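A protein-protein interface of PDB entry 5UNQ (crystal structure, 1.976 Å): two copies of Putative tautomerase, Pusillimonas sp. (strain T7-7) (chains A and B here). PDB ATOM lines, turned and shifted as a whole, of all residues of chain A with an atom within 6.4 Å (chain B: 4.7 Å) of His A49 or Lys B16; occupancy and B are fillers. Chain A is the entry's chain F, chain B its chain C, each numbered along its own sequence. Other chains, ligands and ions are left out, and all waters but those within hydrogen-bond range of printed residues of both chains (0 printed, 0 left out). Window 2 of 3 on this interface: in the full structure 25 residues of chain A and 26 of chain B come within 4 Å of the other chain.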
ATOM      1  N   LEU A  45      -3.777  -3.401  16.101  1.00  0.00           N
ATOM      2  CA  LEU A  45      -2.742  -3.118  17.090  1.00  0.00           C
ATOM      3  C   LEU A  45      -3.294  -3.200  18.510  1.00  0.00           C
ATOM      4  O   LEU A  45      -4.132  -2.389  18.901  1.00  0.00           O
ATOM      5  CB  LEU A  45      -2.135  -1.736  16.845  1.00  0.00           C
ATOM      6  CG  LEU A  45      -1.376  -1.546  15.531  1.00  0.00           C
ATOM      7  CD1 LEU A  45      -1.143  -0.070  15.268  1.00  0.00           C
ATOM      8  CD2 LEU A  45      -0.054  -2.296  15.563  1.00  0.00           C
ATOM      9  N   PRO A  46      -2.822  -4.188  19.286  1.00  0.00           N
ATOM     10  CA  PRO A  46      -3.240  -4.374  20.681  1.00  0.00           C
ATOM     11  C   PRO A  46      -2.820  -3.212  21.577  1.00  0.00           C
ATOM     12  O   PRO A  46      -2.081  -2.330  21.138  1.00  0.00           O
ATOM     13  CB  PRO A  46      -2.522  -5.665  21.095  1.00  0.00           C
ATOM     14  CG  PRO A  46      -2.186  -6.353  19.813  1.00  0.00           C
ATOM     15  CD  PRO A  46      -1.911  -5.254  18.838  1.00  0.00           C
ATOM     16  N   GLY A  47      -3.289  -3.221  22.821  1.00  0.00           N
ATOM     17  CA  GLY A  47      -2.956  -2.176  23.771  1.00  0.00           C
ATOM     18  C   GLY A  47      -1.467  -2.089  24.046  1.00  0.00           C
ATOM     19  O   GLY A  47      -0.810  -3.103  24.286  1.00  0.00           O
ATOM     20  N   GLY A  48      -0.933  -0.872  23.999  1.00  0.00           N
ATOM     21  CA  GLY A  48       0.474  -0.644  24.269  1.00  0.00           C
ATOM     22  C   GLY A  48       1.378  -0.935  23.085  1.00  0.00           C
ATOM     23  O   GLY A  48       2.602  -0.899  23.211  1.00  0.00           O
ATOM     24  N   HIS A  49       0.777  -1.220  21.934  1.00  0.00           N
ATOM     25  CA  HIS A  49       1.541  -1.535  20.729  1.00  0.00           C
ATOM     26  C   HIS A  49       1.550  -0.373  19.740  1.00  0.00           C
ATOM     27  O   HIS A  49       1.960  -0.529  18.590  1.00  0.00           O
ATOM     28  CB  HIS A  49       0.980  -2.787  20.051  1.00  0.00           C
ATOM     29  CG  HIS A  49       1.304  -4.061  20.768  1.00  0.00           C
ATOM     30  ND1 HIS A  49       1.842  -5.158  20.129  1.00  0.00           N
ATOM     31  CD2 HIS A  49       1.172  -4.412  22.069  1.00  0.00           C
ATOM     32  CE1 HIS A  49       2.025  -6.130  21.005  1.00  0.00           C
ATOM     33  NE2 HIS A  49       1.627  -5.703  22.190  1.00  0.00           N
ATOM     34  N   TYR A  50       1.096   0.791  20.192  1.00  0.00           N
ATOM     35  CA  TYR A  50       1.063   1.975  19.343  1.00  0.00           C
ATOM     36  C   TYR A  50       1.453   3.221  20.125  1.00  0.00           C
ATOM     37  O   TYR A  50       0.702   3.692  20.979  1.00  0.00           O
ATOM     38  CB  TYR A  50      -0.325   2.150  18.721  1.00  0.00           C
ATOM     39  CG  TYR A  50      -0.511   3.443  17.956  1.00  0.00           C
ATOM     40  CD1 TYR A  50       0.404   3.841  16.987  1.00  0.00           C
ATOM     41  CD2 TYR A  50      -1.611   4.258  18.191  1.00  0.00           C
ATOM     42  CE1 TYR A  50       0.233   5.021  16.284  1.00  0.00           C
ATOM     43  CE2 TYR A  50      -1.793   5.437  17.492  1.00  0.00           C
ATOM     44  CZ  TYR A  50      -0.868   5.813  16.540  1.00  0.00           C
ATOM     45  OH  TYR A  50      -1.048   6.988  15.846  1.00  0.00           O
ATOM     46  N   LEU A  51       2.638   3.746  19.831  1.00  0.00           N
ATOM     47  CA  LEU A  51       3.108   4.968  20.470  1.00  0.00           C
ATOM     48  C   LEU A  51       2.897   6.159  19.543  1.00  0.00           C
ATOM     49  O   LEU A  51       3.494   6.240  18.469  1.00  0.00           O
ATOM     50  CB  LEU A  51       4.582   4.848  20.859  1.00  0.00           C
ATOM     51  CG  LEU A  51       5.129   6.001  21.703  1.00  0.00           C
ATOM     52  CD1 LEU A  51       4.367   6.106  23.014  1.00  0.00           C
ATOM     53  CD2 LEU A  51       6.616   5.828  21.959  1.00  0.00           C
ATOM     54  N   PHE A  56       0.828   6.642  24.805  1.00  0.00           N
ATOM     55  CA  PHE A  56       0.261   5.317  24.579  1.00  0.00           C
ATOM     56  C   PHE A  56      -1.263   5.375  24.628  1.00  0.00           C
ATOM     57  O   PHE A  56      -1.841   6.413  24.948  1.00  0.00           O
ATOM     58  CB  PHE A  56       0.772   4.315  25.619  1.00  0.00           C
ATOM     59  CG  PHE A  56       2.194   3.877  25.402  1.00  0.00           C
ATOM     60  CD1 PHE A  56       2.493   2.876  24.491  1.00  0.00           C
ATOM     61  CD2 PHE A  56       3.228   4.449  26.124  1.00  0.00           C
ATOM     62  CE1 PHE A  56       3.798   2.464  24.293  1.00  0.00           C
ATOM     63  CE2 PHE A  56       4.537   4.041  25.933  1.00  0.00           C
ATOM     64  CZ  PHE A  56       4.821   3.047  25.015  1.00  0.00           C
ATOM     65  N   LEU B  11       8.745 -11.127  24.916  1.00  0.00           N
ATOM     66  CA  LEU B  11       9.073  -9.930  25.682  1.00  0.00           C
ATOM     67  C   LEU B  11       8.013  -9.612  26.728  1.00  0.00           C
ATOM     68  O   LEU B  11       6.823  -9.844  26.516  1.00  0.00           O
ATOM     69  CB  LEU B  11       9.255  -8.730  24.753  1.00  0.00           C
ATOM     70  CG  LEU B  11      10.482  -8.771  23.841  1.00  0.00           C
ATOM     71  CD1 LEU B  11      10.456  -7.611  22.859  1.00  0.00           C
ATOM     72  CD2 LEU B  11      11.760  -8.754  24.667  1.00  0.00           C
ATOM     73  N   SER B  12       8.459  -9.082  27.862  1.00  0.00           N
ATOM     74  CA  SER B  12       7.554  -8.632  28.908  1.00  0.00           C
ATOM     75  C   SER B  12       6.903  -7.318  28.503  1.00  0.00           C
ATOM     76  O   SER B  12       7.367  -6.651  27.578  1.00  0.00           O
ATOM     77  CB  SER B  12       8.300  -8.459  30.230  1.00  0.00           C
ATOM     78  OG  SER B  12       9.294  -7.455  30.118  1.00  0.00           O
ATOM     79  N   ALA B  13       5.836  -6.947  29.201  1.00  0.00           N
ATOM     80  CA  ALA B  13       5.152  -5.686  28.941  1.00  0.00           C
ATOM     81  C   ALA B  13       6.086  -4.502  29.166  1.00  0.00           C
ATOM     82  O   ALA B  13       6.040  -3.515  28.432  1.00  0.00           O
ATOM     83  CB  ALA B  13       3.914  -5.562  29.816  1.00  0.00           C
ATOM     84  N   GLU B  14       6.935  -4.608  30.185  1.00  0.00           N
ATOM     85  CA  GLU B  14       7.879  -3.545  30.511  1.00  0.00           C
ATOM     86  C   GLU B  14       8.868  -3.297  29.375  1.00  0.00           C
ATOM     87  O   GLU B  14       9.120  -2.151  29.001  1.00  0.00           O
ATOM     88  CB  GLU B  14       8.643  -3.874  31.797  1.00  0.00           C
ATOM     89  CG  GLU B  14       7.845  -3.669  33.078  1.00  0.00           C
ATOM     90  CD  GLU B  14       6.949  -4.846  33.414  1.00  0.00           C
ATOM     91  OE1 GLU B  14       7.053  -5.892  32.739  1.00  0.00           O
ATOM     92  OE2 GLU B  14       6.142  -4.726  34.360  1.00  0.00           O
ATOM     93  N   LYS B  15       9.429  -4.373  28.834  1.00  0.00           N
ATOM     94  CA  LYS B  15      10.405  -4.260  27.757  1.00  0.00           C
ATOM     95  C   LYS B  15       9.755  -3.781  26.463  1.00  0.00           C
ATOM     96  O   LYS B  15      10.384  -3.070  25.677  1.00  0.00           O
ATOM     97  CB  LYS B  15      11.120  -5.594  27.534  1.00  0.00           C
ATOM     98  CG  LYS B  15      12.317  -5.798  28.449  1.00  0.00           C
ATOM     99  CD  LYS B  15      13.055  -7.087  28.142  1.00  0.00           C
ATOM    100  CE  LYS B  15      14.485  -7.030  28.657  1.00  0.00           C
ATOM    101  NZ  LYS B  15      14.564  -6.447  30.028  1.00  0.00           N
ATOM    102  N   LYS B  16       8.502  -4.171  26.245  1.00  0.00           N
ATOM    103  CA  LYS B  16       7.730  -3.661  25.116  1.00  0.00           C
ATOM    104  C   LYS B  16       7.587  -2.152  25.233  1.00  0.00           C
ATOM    105  O   LYS B  16       7.815  -1.416  24.274  1.00  0.00           O
ATOM    106  CB  LYS B  16       6.344  -4.307  25.051  1.00  0.00           C
ATOM    107  CG  LYS B  16       6.329  -5.781  24.693  1.00  0.00           C
ATOM    108  CD  LYS B  16       4.895  -6.289  24.651  1.00  0.00           C
ATOM    109  CE  LYS B  16       4.828  -7.798  24.504  1.00  0.00           C
ATOM    110  NZ  LYS B  16       3.418  -8.278  24.544  1.00  0.00           N
ATOM    111  N   LYS B  17       7.207  -1.704  26.426  1.00  0.00           N
ATOM    112  CA  LYS B  17       7.066  -0.285  26.720  1.00  0.00           C
ATOM    113  C   LYS B  17       8.391   0.442  26.511  1.00  0.00           C
ATOM    114  O   LYS B  17       8.431   1.529  25.936  1.00  0.00           O
ATOM    115  CB  LYS B  17       6.571  -0.088  28.155  1.00  0.00           C
ATOM    116  CG  LYS B  17       6.223   1.343  28.515  1.00  0.00           C
ATOM    117  CD  LYS B  17       5.786   1.446  29.968  1.00  0.00           C
ATOM    118  CE  LYS B  17       5.419   2.874  30.337  1.00  0.00           C
ATOM    119  NZ  LYS B  17       5.084   3.005  31.784  1.00  0.00           N
ATOM    120  N   GLN B  18       9.472  -0.174  26.982  1.00  0.00           N
ATOM    121  CA  GLN B  18      10.814   0.377  26.823  1.00  0.00           C
ATOM    122  C   GLN B  18      11.218   0.460  25.355  1.00  0.00           C
ATOM    123  O   GLN B  18      11.807   1.450  24.918  1.00  0.00           O
ATOM    124  CB  GLN B  18      11.833  -0.467  27.592  1.00  0.00           C
ATOM    125  CG  GLN B  18      11.850  -0.215  29.089  1.00  0.00           C
ATOM    126  CD  GLN B  18      12.348   1.174  29.433  1.00  0.00           C
ATOM    127  OE1 GLN B  18      11.583   2.024  29.888  1.00  0.00           O
ATOM    128  NE2 GLN B  18      13.638   1.412  29.215  1.00  0.00           N
ATOM    129  N   LEU B  19      10.902  -0.590  24.604  1.00  0.00           N
ATOM    130  CA  LEU B  19      11.272  -0.671  23.196  1.00  0.00           C
ATOM    131  C   LEU B  19      10.693   0.488  22.390  1.00  0.00           C
ATOM    132  O   LEU B  19      11.416   1.163  21.660  1.00  0.00           O
ATOM    133  CB  LEU B  19      10.817  -2.007  22.602  1.00  0.00           C
ATOM    134  CG  LEU B  19      11.127  -2.262  21.124  1.00  0.00           C
ATOM    135  CD1 LEU B  19      12.606  -2.060  20.835  1.00  0.00           C
ATOM    136  CD2 LEU B  19      10.692  -3.664  20.725  1.00  0.00           C
ATOM    137  N   LEU B  20       9.394   0.729  22.541  1.00  0.00           N
ATOM    138  CA  LEU B  20       8.723   1.772  21.773  1.00  0.00           C
ATOM    139  C   LEU B  20       9.130   3.176  22.218  1.00  0.00           C
ATOM    140  O   LEU B  20       9.345   4.056  21.384  1.00  0.00           O
ATOM    141  CB  LEU B  20       7.203   1.613  21.864  1.00  0.00           C
ATOM    142  CG  LEU B  20       6.551   0.714  20.806  1.00  0.00           C
ATOM    143  CD1 LEU B  20       6.939  -0.749  20.987  1.00  0.00           C
ATOM    144  CD2 LEU B  20       5.036   0.875  20.809  1.00  0.00           C
ATOM    145  N   VAL B  40       5.235   4.940  16.509  1.00  0.00           N
ATOM    146  CA  VAL B  40       5.855   3.622  16.588  1.00  0.00           C
ATOM    147  C   VAL B  40       4.795   2.532  16.721  1.00  0.00           C
ATOM    148  O   VAL B  40       3.956   2.577  17.620  1.00  0.00           O
ATOM    149  CB  VAL B  40       6.835   3.513  17.775  1.00  0.00           C
ATOM    150  CG1 VAL B  40       7.618   2.213  17.690  1.00  0.00           C
ATOM    151  CG2 VAL B  40       7.787   4.701  17.802  1.00  0.00           C
ATOM    152  N   MET B  41       4.833   1.559  15.817  1.00  0.00           N
ATOM    153  CA  MET B  41       3.898   0.439  15.851  1.00  0.00           C
ATOM    154  C   MET B  41       4.636  -0.873  16.090  1.00  0.00           C
ATOM    155  O   MET B  41       5.756  -1.060  15.614  1.00  0.00           O
ATOM    156  CB  MET B  41       3.093   0.363  14.549  1.00  0.00           C
ATOM    157  CG  MET B  41       2.018   1.433  14.408  1.00  0.00           C
ATOM    158  SD  MET B  41       2.667   3.092  14.120  1.00  0.00           S
ATOM    159  CE  MET B  41       3.428   2.882  12.512  1.00  0.00           C
ATOM    160  N   LEU B  42       4.002  -1.780  16.826  1.00  0.00           N
ATOM    161  CA  LEU B  42       4.618  -3.057  17.168  1.00  0.00           C
ATOM    162  C   LEU B  42       3.746  -4.241  16.755  1.00  0.00           C
ATOM    163  O   LEU B  42       2.565  -4.306  17.099  1.00  0.00           O
ATOM    164  CB  LEU B  42       4.907  -3.122  18.671  1.00  0.00           C
ATOM    165  CG  LEU B  42       5.421  -4.451  19.231  1.00  0.00           C
ATOM    166  CD1 LEU B  42       6.770  -4.819  18.632  1.00  0.00           C
ATOM    167  CD2 LEU B  42       5.503  -4.396  20.752  1.00  0.00           C
ATOM    168  N   GLU B  44       3.770  -8.450  16.946  1.00  0.00           N
ATOM    169  CA  GLU B  44       4.430  -9.576  17.592  1.00  0.00           C
ATOM    170  C   GLU B  44       4.269 -10.853  16.772  1.00  0.00           C
ATOM    171  O   GLU B  44       3.162 -11.208  16.366  1.00  0.00           O
ATOM    172  CB  GLU B  44       3.878  -9.771  19.007  1.00  0.00           C
ATOM    173  CG  GLU B  44       4.886 -10.317  20.003  1.00  0.00           C
ATOM    174  CD  GLU B  44       4.504 -10.009  21.440  1.00  0.00           C
ATOM    175  OE1 GLU B  44       5.221 -10.459  22.358  1.00  0.00           O
ATOM    176  OE2 GLU B  44       3.490  -9.312  21.651  1.00  0.00           O
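Of chain B, only Lys B16 (3.9 Å), Leu B20 (3.9 Å), Val B40 (3.8 Å), Met B41 (3.5 Å), Leu B42 (3.0 Å) and Glu B44 (3.6 Å) come within 4 Å of His A49. Lys B16 touches just one residue of chain A: His A49. Of the printed residues of chain A, Met B41 touches Leu A45 (3.6 Å), His A49 (3.5 Å) and Tyr A50 (3.7 Å). Printed residues of chain B within 4 Å of Leu A51: Leu B20 (3.3 Å) and Val B40 (2.8 Å). Of the printed residues of chain B, Gly A48 touches Leu B20 (3.9 Å). Leu B11 touches none of the printed residues of chain A. Pro A46 touches none of the printed residues of chain B. The nearest printed residue of chain B that does not touch His A49 is Ala B13 (7.6 Å). The nearest residue of chain A that does not touch Lys B16 is Gly A48 (5.3 Å). The nearest printed residue of chain A that does not touch Met B41 is Leu A51 (5.1 Å).
O of His A49 sits at hydrogen-bond distance from N of Leu B42 (3.0 Å). The backbone NH (N) of Leu A51 is in hydrogen-bond range of the backbone carbonyl oxygen (O) of Val B40 (2.8 Å).
NZ of Lys B16 is in salt-bridge range of OE2 of Glu B44, 3.1 Å away.
No position is printed for both chains.
Hydrophobic or aromatic side chains of chain A within 4 Å of the printed part of chain B: Leu A45, His A49, Tyr A50 and Leu A51. Of the 14 printed residues of chain B, 6 touch a printed residue of chain A. Along chain B the printed residues that touch a printed residue of chain A span positions 16 to 44. Among the printed residues, 14 pairs touch across the chains.
Among the printed residues, pairs that only touch across the chains: Leu A51 with Leu B20 (3.3 Å), Tyr A50 with Val B40 (3.4 Å), His A49 with Met B41 (3.5 Å), His A49 with Glu B44 (3.6 Å), Leu A45 with Met B41 (3.6 Å), Leu A45 with Leu B42 (3.6 Å), Tyr A50 with Met B41 (3.7 Å), His A49 with Val B40 (3.8 Å), Gly A48 with Leu B20 (3.9 Å), His A49 with Leu B20 (3.9 Å), His A49 with Lys B16 (3.9 Å) and Tyr A50 with Leu B20 (3.99 Å).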
